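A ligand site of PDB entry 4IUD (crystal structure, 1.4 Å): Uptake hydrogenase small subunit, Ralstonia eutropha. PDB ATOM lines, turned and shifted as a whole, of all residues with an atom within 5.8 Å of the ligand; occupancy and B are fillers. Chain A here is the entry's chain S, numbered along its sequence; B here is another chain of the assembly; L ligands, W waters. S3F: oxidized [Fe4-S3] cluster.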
ATOM      1  N   LEU A  15     -27.169 -16.204 -31.962  1.00  0.00           N
ATOM      2  CA  LEU A  15     -26.163 -16.643 -30.976  1.00  0.00           C
ATOM      3  C   LEU A  15     -26.697 -16.281 -29.596  1.00  0.00           C
ATOM      4  O   LEU A  15     -26.996 -15.126 -29.336  1.00  0.00           O
ATOM      5  CB  LEU A  15     -24.806 -15.988 -31.221  1.00  0.00           C
ATOM      6  CG  LEU A  15     -24.062 -16.412 -32.496  1.00  0.00           C
ATOM      7  CD1 LEU A  15     -22.724 -15.691 -32.585  1.00  0.00           C
ATOM      8  CD2 LEU A  15     -23.873 -17.918 -32.546  1.00  0.00           C
ATOM      9  N   GLU A  16     -26.776 -17.277 -28.723  1.00  0.00           N
ATOM     10  CA  GLU A  16     -27.481 -17.156 -27.457  1.00  0.00           C
ATOM     11  C   GLU A  16     -27.091 -18.299 -26.532  1.00  0.00           C
ATOM     12  O   GLU A  16     -26.463 -19.253 -26.960  1.00  0.00           O
ATOM     13  CB  GLU A  16     -28.979 -17.232 -27.704  1.00  0.00           C
ATOM     14  CG  GLU A  16     -29.467 -18.610 -28.130  1.00  0.00           C
ATOM     15  CD  GLU A  16     -30.954 -18.661 -28.287  1.00  0.00           C
ATOM     16  OE1 GLU A  16     -31.536 -17.663 -28.762  1.00  0.00           O
ATOM     17  OE2 GLU A  16     -31.554 -19.697 -27.940  1.00  0.00           O
ATOM     18  N   CYS A  17     -27.498 -18.190 -25.262  1.00  0.00           N
ATOM     19  CA  CYS A  17     -27.399 -19.295 -24.316  1.00  0.00           C
ATOM     20  C   CYS A  17     -28.780 -19.822 -23.898  1.00  0.00           C
ATOM     21  O   CYS A  17     -28.866 -20.769 -23.124  1.00  0.00           O
ATOM     22  CB  CYS A  17     -26.660 -18.857 -23.058  1.00  0.00           C
ATOM     23  SG  CYS A  17     -27.703 -18.114 -21.792  1.00  0.00           S
ATOM     24  N   THR A  18     -29.844 -19.184 -24.416  1.00  0.00           N
ATOM     25  CA  THR A  18     -31.256 -19.567 -24.174  1.00  0.00           C
ATOM     26  C   THR A  18     -31.803 -19.188 -22.771  1.00  0.00           C
ATOM     27  O   THR A  18     -32.892 -19.600 -22.393  1.00  0.00           O
ATOM     28  CB  THR A  18     -31.476 -21.064 -24.537  1.00  0.00           C
ATOM     29  OG1 THR A  18     -30.846 -21.320 -25.796  1.00  0.00           O
ATOM     30  CG2 THR A  18     -32.945 -21.405 -24.668  1.00  0.00           C
ATOM     31  N   CYS A  19     -31.066 -18.350 -22.033  1.00  0.00           N
ATOM     32  CA  CYS A  19     -31.546 -17.900 -20.712  1.00  0.00           C
ATOM     33  C   CYS A  19     -32.834 -17.088 -20.787  1.00  0.00           C
ATOM     34  O   CYS A  19     -33.654 -17.150 -19.867  1.00  0.00           O
ATOM     35  CB  CYS A  19     -30.475 -17.120 -19.921  1.00  0.00           C
ATOM     36  SG  CYS A  19     -29.962 -15.491 -20.556  1.00  0.00           S
ATOM     37  N   CYS A  20     -33.038 -16.352 -21.867  1.00  0.00           N
ATOM     38  CA  CYS A  20     -34.215 -15.484 -21.975  1.00  0.00           C
ATOM     39  C   CYS A  20     -35.476 -16.323 -22.173  1.00  0.00           C
ATOM     40  O   CYS A  20     -36.507 -16.062 -21.555  1.00  0.00           O
ATOM     41  CB  CYS A  20     -34.032 -14.444 -23.087  1.00  0.00           C
ATOM     42  SG  CYS A  20     -32.536 -13.443 -22.882  1.00  0.00           S
ATOM     43  N   GLU A  76     -34.171 -13.474 -29.618  1.00  0.00           N
ATOM     44  CA  GLU A  76     -33.252 -13.877 -28.567  1.00  0.00           C
ATOM     45  C   GLU A  76     -31.912 -14.133 -29.232  1.00  0.00           C
ATOM     46  O   GLU A  76     -31.853 -14.727 -30.308  1.00  0.00           O
ATOM     47  CB  GLU A  76     -33.767 -15.137 -27.899  1.00  0.00           C
ATOM     48  CG  GLU A  76     -32.955 -15.646 -26.716  1.00  0.00           C
ATOM     49  CD  GLU A  76     -33.695 -16.717 -25.944  1.00  0.00           C
ATOM     50  OE1 GLU A  76     -34.838 -17.057 -26.314  1.00  0.00           O
ATOM     51  OE2 GLU A  76     -33.143 -17.222 -24.951  1.00  0.00           O
ATOM     52  N   GLY A  77     -30.838 -13.676 -28.616  1.00  0.00           N
ATOM     53  CA  GLY A  77     -29.533 -13.807 -29.218  1.00  0.00           C
ATOM     54  C   GLY A  77     -29.257 -12.749 -30.251  1.00  0.00           C
ATOM     55  O   GLY A  77     -29.992 -11.766 -30.378  1.00  0.00           O
ATOM     56  N   TRP A 112     -35.011  -9.357 -26.976  1.00  0.00           N
ATOM     57  CA  TRP A 112     -34.960  -9.997 -25.648  1.00  0.00           C
ATOM     58  C   TRP A 112     -33.562 -10.066 -25.130  1.00  0.00           C
ATOM     59  O   TRP A 112     -32.661 -10.553 -25.815  1.00  0.00           O
ATOM     60  CB  TRP A 112     -35.421 -11.458 -25.702  1.00  0.00           C
ATOM     61  CG  TRP A 112     -36.894 -11.738 -25.871  1.00  0.00           C
ATOM     62  CD1 TRP A 112     -37.461 -12.691 -26.712  1.00  0.00           C
ATOM     63  CD2 TRP A 112     -38.019 -11.145 -25.146  1.00  0.00           C
ATOM     64  NE1 TRP A 112     -38.825 -12.710 -26.568  1.00  0.00           N
ATOM     65  CE2 TRP A 112     -39.217 -11.815 -25.644  1.00  0.00           C
ATOM     66  CE3 TRP A 112     -38.150 -10.166 -24.168  1.00  0.00           C
ATOM     67  CZ2 TRP A 112     -40.486 -11.494 -25.180  1.00  0.00           C
ATOM     68  CZ3 TRP A 112     -39.446  -9.849 -23.708  1.00  0.00           C
ATOM     69  CH2 TRP A 112     -40.574 -10.500 -24.210  1.00  0.00           C
ATOM     70  N   GLY A 113     -33.372  -9.617 -23.884  1.00  0.00           N
ATOM     71  CA  GLY A 113     -32.111  -9.820 -23.184  1.00  0.00           C
ATOM     72  C   GLY A 113     -30.954  -8.985 -23.669  1.00  0.00           C
ATOM     73  O   GLY A 113     -31.045  -8.262 -24.675  1.00  0.00           O
ATOM     74  N   SER A 114     -29.848  -9.080 -22.960  1.00  0.00           N
ATOM     75  CA  SER A 114     -28.665  -8.337 -23.290  1.00  0.00           C
ATOM     76  C   SER A 114     -28.053  -8.771 -24.634  1.00  0.00           C
ATOM     77  O   SER A 114     -27.443  -7.953 -25.307  1.00  0.00           O
ATOM     78  CB  SER A 114     -27.650  -8.445 -22.164  1.00  0.00           C
ATOM     79  OG  SER A 114     -28.180  -7.756 -21.030  1.00  0.00           O
ATOM     80  N   CYS A 115     -28.218 -10.039 -25.014  1.00  0.00           N
ATOM     81  CA  CYS A 115     -27.695 -10.518 -26.303  1.00  0.00           C
ATOM     82  C   CYS A 115     -28.279  -9.688 -27.449  1.00  0.00           C
ATOM     83  O   CYS A 115     -27.544  -9.066 -28.223  1.00  0.00           O
ATOM     84  CB  CYS A 115     -28.016 -11.993 -26.542  1.00  0.00           C
ATOM     85  SG  CYS A 115     -26.915 -13.191 -25.772  1.00  0.00           S
ATOM     86  N   ALA A 116     -29.603  -9.688 -27.537  1.00  0.00           N
ATOM     87  CA  ALA A 116     -30.272  -9.005 -28.650  1.00  0.00           C
ATOM     88  C   ALA A 116     -30.149  -7.503 -28.509  1.00  0.00           C
ATOM     89  O   ALA A 116     -30.015  -6.796 -29.504  1.00  0.00           O
ATOM     90  CB  ALA A 116     -31.727  -9.429 -28.744  1.00  0.00           C
ATOM     91  N   CYS A 120     -24.103  -8.853 -25.271  1.00  0.00           N
ATOM     92  CA  CYS A 120     -23.819  -9.748 -24.130  1.00  0.00           C
ATOM     93  C   CYS A 120     -22.478 -10.508 -24.264  1.00  0.00           C
ATOM     94  O   CYS A 120     -21.525  -9.969 -24.824  1.00  0.00           O
ATOM     95  CB  CYS A 120     -25.006 -10.683 -23.831  1.00  0.00           C
ATOM     96  SG  CYS A 120     -25.080 -11.243 -22.100  1.00  0.00           S
ATOM     97  N   VAL A 121     -22.397 -11.724 -23.750  1.00  0.00           N
ATOM     98  CA  VAL A 121     -21.093 -12.326 -23.461  1.00  0.00           C
ATOM     99  C   VAL A 121     -20.255 -12.573 -24.723  1.00  0.00           C
ATOM    100  O   VAL A 121     -19.050 -12.328 -24.709  1.00  0.00           O
ATOM    101  CB  VAL A 121     -21.229 -13.610 -22.602  1.00  0.00           C
ATOM    102  CG1 VAL A 121     -21.735 -14.788 -23.435  1.00  0.00           C
ATOM    103  CG2 VAL A 121     -19.916 -13.943 -21.925  1.00  0.00           C
ATOM    104  N   GLN A 122     -20.900 -13.008 -25.797  1.00  0.00           N
ATOM    105  CA  GLN A 122     -20.177 -13.251 -27.064  1.00  0.00           C
ATOM    106  C   GLN A 122     -19.593 -11.972 -27.681  1.00  0.00           C
ATOM    107  O   GLN A 122     -18.663 -12.045 -28.488  1.00  0.00           O
ATOM    108  CB  GLN A 122     -21.051 -13.988 -28.095  1.00  0.00           C
ATOM    109  CG  GLN A 122     -22.366 -13.298 -28.446  1.00  0.00           C
ATOM    110  CD  GLN A 122     -23.524 -13.770 -27.604  1.00  0.00           C
ATOM    111  OE1 GLN A 122     -23.363 -14.113 -26.432  1.00  0.00           O
ATOM    112  NE2 GLN A 122     -24.719 -13.782 -28.189  1.00  0.00           N
ATOM    113  N   GLY A 148     -30.845  -7.393 -19.813  1.00  0.00           N
ATOM    114  CA  GLY A 148     -30.711  -8.264 -18.659  1.00  0.00           C
ATOM    115  C   GLY A 148     -30.274  -9.639 -19.130  1.00  0.00           C
ATOM    116  O   GLY A 148     -30.611 -10.064 -20.240  1.00  0.00           O
ATOM    117  N   CYS A 149     -29.539 -10.349 -18.288  1.00  0.00           N
ATOM    118  CA  CYS A 149     -28.987 -11.636 -18.649  1.00  0.00           C
ATOM    119  C   CYS A 149     -29.380 -12.718 -17.631  1.00  0.00           C
ATOM    120  O   CYS A 149     -28.598 -13.067 -16.731  1.00  0.00           O
ATOM    121  CB  CYS A 149     -27.467 -11.529 -18.763  1.00  0.00           C
ATOM    122  SG  CYS A 149     -26.745 -13.026 -19.463  1.00  0.00           S
ATOM    123  N   PRO A 150     -30.615 -13.241 -17.746  1.00  0.00           N
ATOM    124  CA  PRO A 150     -31.697 -12.790 -18.621  1.00  0.00           C
ATOM    125  C   PRO A 150     -32.468 -11.669 -17.940  1.00  0.00           C
ATOM    126  O   PRO A 150     -32.161 -11.329 -16.789  1.00  0.00           O
ATOM    127  CB  PRO A 150     -32.573 -14.020 -18.739  1.00  0.00           C
ATOM    128  CG  PRO A 150     -32.414 -14.731 -17.436  1.00  0.00           C
ATOM    129  CD  PRO A 150     -31.059 -14.355 -16.881  1.00  0.00           C
ATOM    130  N   PRO A 151     -33.460 -11.094 -18.636  1.00  0.00           N
ATOM    131  CA  PRO A 151     -34.386 -10.200 -17.950  1.00  0.00           C
ATOM    132  C   PRO A 151     -35.229 -10.967 -16.940  1.00  0.00           C
ATOM    133  O   PRO A 151     -35.349 -12.195 -17.039  1.00  0.00           O
ATOM    134  CB  PRO A 151     -35.278  -9.650 -19.079  1.00  0.00           C
ATOM    135  CG  PRO A 151     -34.625 -10.049 -20.351  1.00  0.00           C
ATOM    136  CD  PRO A 151     -33.803 -11.253 -20.058  1.00  0.00           C
ATOM    137  N   PHE A 257     -21.460  -4.668 -20.092  1.00  0.00           N
ATOM    138  CA  PHE A 257     -21.138  -4.903 -18.666  1.00  0.00           C
ATOM    139  C   PHE A 257     -19.994  -5.888 -18.428  1.00  0.00           C
ATOM    140  O   PHE A 257     -19.390  -5.889 -17.369  1.00  0.00           O
ATOM    141  CB  PHE A 257     -22.390  -5.302 -17.853  1.00  0.00           C
ATOM    142  CG  PHE A 257     -22.888  -6.708 -18.093  1.00  0.00           C
ATOM    143  CD1 PHE A 257     -23.787  -6.973 -19.137  1.00  0.00           C
ATOM    144  CD2 PHE A 257     -22.522  -7.756 -17.246  1.00  0.00           C
ATOM    145  CE1 PHE A 257     -24.273  -8.259 -19.336  1.00  0.00           C
ATOM    146  CE2 PHE A 257     -23.004  -9.049 -17.462  1.00  0.00           C
ATOM    147  CZ  PHE A 257     -23.894  -9.292 -18.492  1.00  0.00           C
ATOM    148  N   TRP A 258     -19.700  -6.731 -19.427  1.00  0.00           N
ATOM    149  CA  TRP A 258     -18.587  -7.685 -19.341  1.00  0.00           C
ATOM    150  C   TRP A 258     -17.227  -7.021 -19.424  1.00  0.00           C
ATOM    151  O   TRP A 258     -16.230  -7.598 -19.001  1.00  0.00           O
ATOM    152  CB  TRP A 258     -18.670  -8.718 -20.476  1.00  0.00           C
ATOM    153  CG  TRP A 258     -19.958  -9.511 -20.456  1.00  0.00           C
ATOM    154  CD1 TRP A 258     -21.079  -9.349 -21.274  1.00  0.00           C
ATOM    155  CD2 TRP A 258     -20.286 -10.611 -19.561  1.00  0.00           C
ATOM    156  NE1 TRP A 258     -22.048 -10.261 -20.949  1.00  0.00           N
ATOM    157  CE2 TRP A 258     -21.626 -11.048 -19.922  1.00  0.00           C
ATOM    158  CE3 TRP A 258     -19.616 -11.262 -18.537  1.00  0.00           C
ATOM    159  CZ2 TRP A 258     -22.267 -12.083 -19.264  1.00  0.00           C
ATOM    160  CZ3 TRP A 258     -20.263 -12.305 -17.877  1.00  0.00           C
ATOM    161  CH2 TRP A 258     -21.558 -12.712 -18.230  1.00  0.00           C
ATOM    162  N   ARG B  53     -19.584 -19.171 -30.390  1.00  0.00           N
ATOM    163  CA  ARG B  53     -19.459 -17.839 -29.769  1.00  0.00           C
ATOM    164  C   ARG B  53     -18.030 -17.489 -29.341  1.00  0.00           C
ATOM    165  O   ARG B  53     -17.654 -16.327 -29.336  1.00  0.00           O
ATOM    166  CB  ARG B  53     -20.412 -17.724 -28.576  1.00  0.00           C
ATOM    167  CG  ARG B  53     -21.875 -17.534 -28.982  1.00  0.00           C
ATOM    168  CD  ARG B  53     -22.811 -17.714 -27.795  1.00  0.00           C
ATOM    169  NE  ARG B  53     -22.690 -19.069 -27.270  1.00  0.00           N
ATOM    170  CZ  ARG B  53     -22.988 -19.461 -26.034  1.00  0.00           C
ATOM    171  NH1 ARG B  53     -23.475 -18.612 -25.145  1.00  0.00           N
ATOM    172  NH2 ARG B  53     -22.779 -20.732 -25.691  1.00  0.00           N
ATOM    173  N   ARG B  73     -22.705 -18.243 -18.802  1.00  0.00           N
ATOM    174  CA  ARG B  73     -23.462 -17.821 -19.982  1.00  0.00           C
ATOM    175  C   ARG B  73     -23.145 -18.649 -21.236  1.00  0.00           C
ATOM    176  O   ARG B  73     -23.610 -18.335 -22.329  1.00  0.00           O
ATOM    177  CB  ARG B  73     -23.247 -16.320 -20.251  1.00  0.00           C
ATOM    178  CG  ARG B  73     -24.208 -15.418 -19.487  1.00  0.00           C
ATOM    179  CD  ARG B  73     -24.013 -15.471 -17.975  1.00  0.00           C
ATOM    180  NE  ARG B  73     -24.906 -14.508 -17.333  1.00  0.00           N
ATOM    181  CZ  ARG B  73     -24.908 -14.180 -16.044  1.00  0.00           C
ATOM    182  NH1 ARG B  73     -24.032 -14.725 -15.187  1.00  0.00           N
ATOM    183  NH2 ARG B  73     -25.807 -13.301 -15.611  1.00  0.00           N
ATOM    184  N   CYS B  75     -24.556 -21.376 -21.266  1.00  0.00           N
ATOM    185  CA  CYS B  75     -25.858 -21.999 -21.365  1.00  0.00           C
ATOM    186  C   CYS B  75     -26.810 -21.631 -20.233  1.00  0.00           C
ATOM    187  O   CYS B  75     -26.475 -21.738 -19.066  1.00  0.00           O
ATOM    188  CB  CYS B  75     -25.714 -23.503 -21.403  1.00  0.00           C
ATOM    189  SG  CYS B  75     -27.242 -24.281 -21.906  1.00  0.00           S
ATOM    190  N   GLY B  76     -28.009 -21.194 -20.618  1.00  0.00           N
ATOM    191  CA  GLY B  76     -29.070 -20.841 -19.658  1.00  0.00           C
ATOM    192  C   GLY B  76     -30.039 -21.975 -19.362  1.00  0.00           C
ATOM    193  O   GLY B  76     -30.936 -21.805 -18.533  1.00  0.00           O
ATOM    194  N   HIS B 229     -29.291 -18.309 -14.288  1.00  0.00           N
ATOM    195  CA  HIS B 229     -27.985 -17.713 -14.000  1.00  0.00           C
ATOM    196  C   HIS B 229     -27.766 -17.260 -12.572  1.00  0.00           C
ATOM    197  O   HIS B 229     -27.424 -16.091 -12.312  1.00  0.00           O
ATOM    198  CB  HIS B 229     -27.656 -16.611 -14.996  1.00  0.00           C
ATOM    199  CG  HIS B 229     -27.454 -17.108 -16.391  1.00  0.00           C
ATOM    200  ND1 HIS B 229     -27.021 -18.367 -16.667  1.00  0.00           N
ATOM    201  CD2 HIS B 229     -27.622 -16.475 -17.608  1.00  0.00           C
ATOM    202  CE1 HIS B 229     -26.918 -18.512 -17.999  1.00  0.00           C
ATOM    203  NE2 HIS B 229     -27.275 -17.369 -18.574  1.00  0.00           N
HETATM  204  S2  S3F L   1     -26.370 -14.819 -22.700  1.00  0.00           S
HETATM  205 FE2  S3F L   1     -28.044 -13.932 -23.917  1.00  0.00          FE
HETATM  206  S3  S3F L   1     -28.876 -12.375 -22.559  1.00  0.00           S
HETATM  207 FE3  S3F L   1     -26.808 -12.835 -21.733  1.00  0.00          FE
HETATM  208  S1  S3F L   1     -29.604 -15.601 -24.189  1.00  0.00           S
HETATM  209 FE1  S3F L   1     -28.251 -15.941 -22.363  1.00  0.00          FE
HETATM  210  O1  S3F L   1     -27.889 -16.241 -20.613  1.00  0.00           O
HETATM  211 FE4  S3F L   1     -30.387 -14.348 -22.527  1.00  0.00          FE
HETATM  212  O   HOH W   1     -24.885 -16.155 -25.468  1.00  0.00           O
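N of Cys 19 lies close to S1 of the ligand (3.8 Å).
SG of Cys 19 is bound to FE4 of the ligand (2.3 Å).
The backbone NH (N) of Cys 17 lies close to a sulfur (S1) of the ligand (3.5 Å).
The side-chain sulfur (SG) of Cys 17 is bound to an iron atom (FE1) of the ligand, 2.3 Å away.
The side-chain sulfur (SG) of Cys 149 binds an iron atom (FE3) of the ligand (2.3 Å).
The backbone NH (N) of Cys 115 lies close to a sulfur (S3) of the ligand, 3.5 Å away.
SG of Cys 115 binds FE2 of the ligand (2.3 Å).
The side-chain sulfur (SG) of Cys 20 binds an iron atom (FE4) of the ligand, 2.4 Å away.
FE3 of the ligand is bound by SG of Cys 120.
A ring nitrogen (NE2) of His 229 of chain B sits close to an oxygen (O1) of the ligand (2.4 Å).
The backbone NH (N) of Ser 114 lies close to a sulfur (S3) of the ligand (3.5 Å).
The backbone NH of Thr 18 sits close to a sulfur (S1) of the ligand (3.6 Å).
The side-chain sulfur (SG) of Cys 17 sits close to a ring nitrogen (NE2) of His 229 of chain B, at 3.3 Å.
NH2 of Arg 73 of chain B is in hydrogen-bond range of O of Cys 149 (3.0 Å).
SG of Cys 115 sits close to NE2 of Gln 122.
N of Cys 20 lies within hydrogen-bond range of OE2 of Glu 76 of chain A (3.2 Å).
NE1 of Trp 258 lies close to SG of Cys 120, 3.4 Å away.
The side-chain hydroxyl (OG) of Ser 114 lies within hydrogen-bond range of the backbone NH (N) of Gly 148 (3.0 Å).
OG1 of Thr 18 sits at hydrogen-bond distance from OE2 of Glu 16 (2.8 Å).
NH1 of Arg 53 of chain B is in hydrogen-bond range of O of Arg 73 of chain B (2.8 Å).
O of Gly 148 sits close to S3 of the ligand, 3.7 Å away.
Merely in contact with the ligand: Arg 73 of chain B (3.9 Å), Glu 16 (3.9 Å) and Glu 76 of chain A (3.97 Å).
Within 4 Å of the ligand: Glu 16, Cys 17, Thr 18, Cys 19, Cys 20, Glu 76 of chain A, Ser 114, Cys 115, Cys 120, Gly 148, Cys 149, Arg 73 of chain B and His 229 of chain B.
The nearest printed residue that does not touch the ligand is Gly 113 (4.1 Å).
Water W1 lies within hydrogen-bond range of OE1 of Gln 122, NH1 of Arg 53 of chain B, N of Cys 17 and S2 of the ligand.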
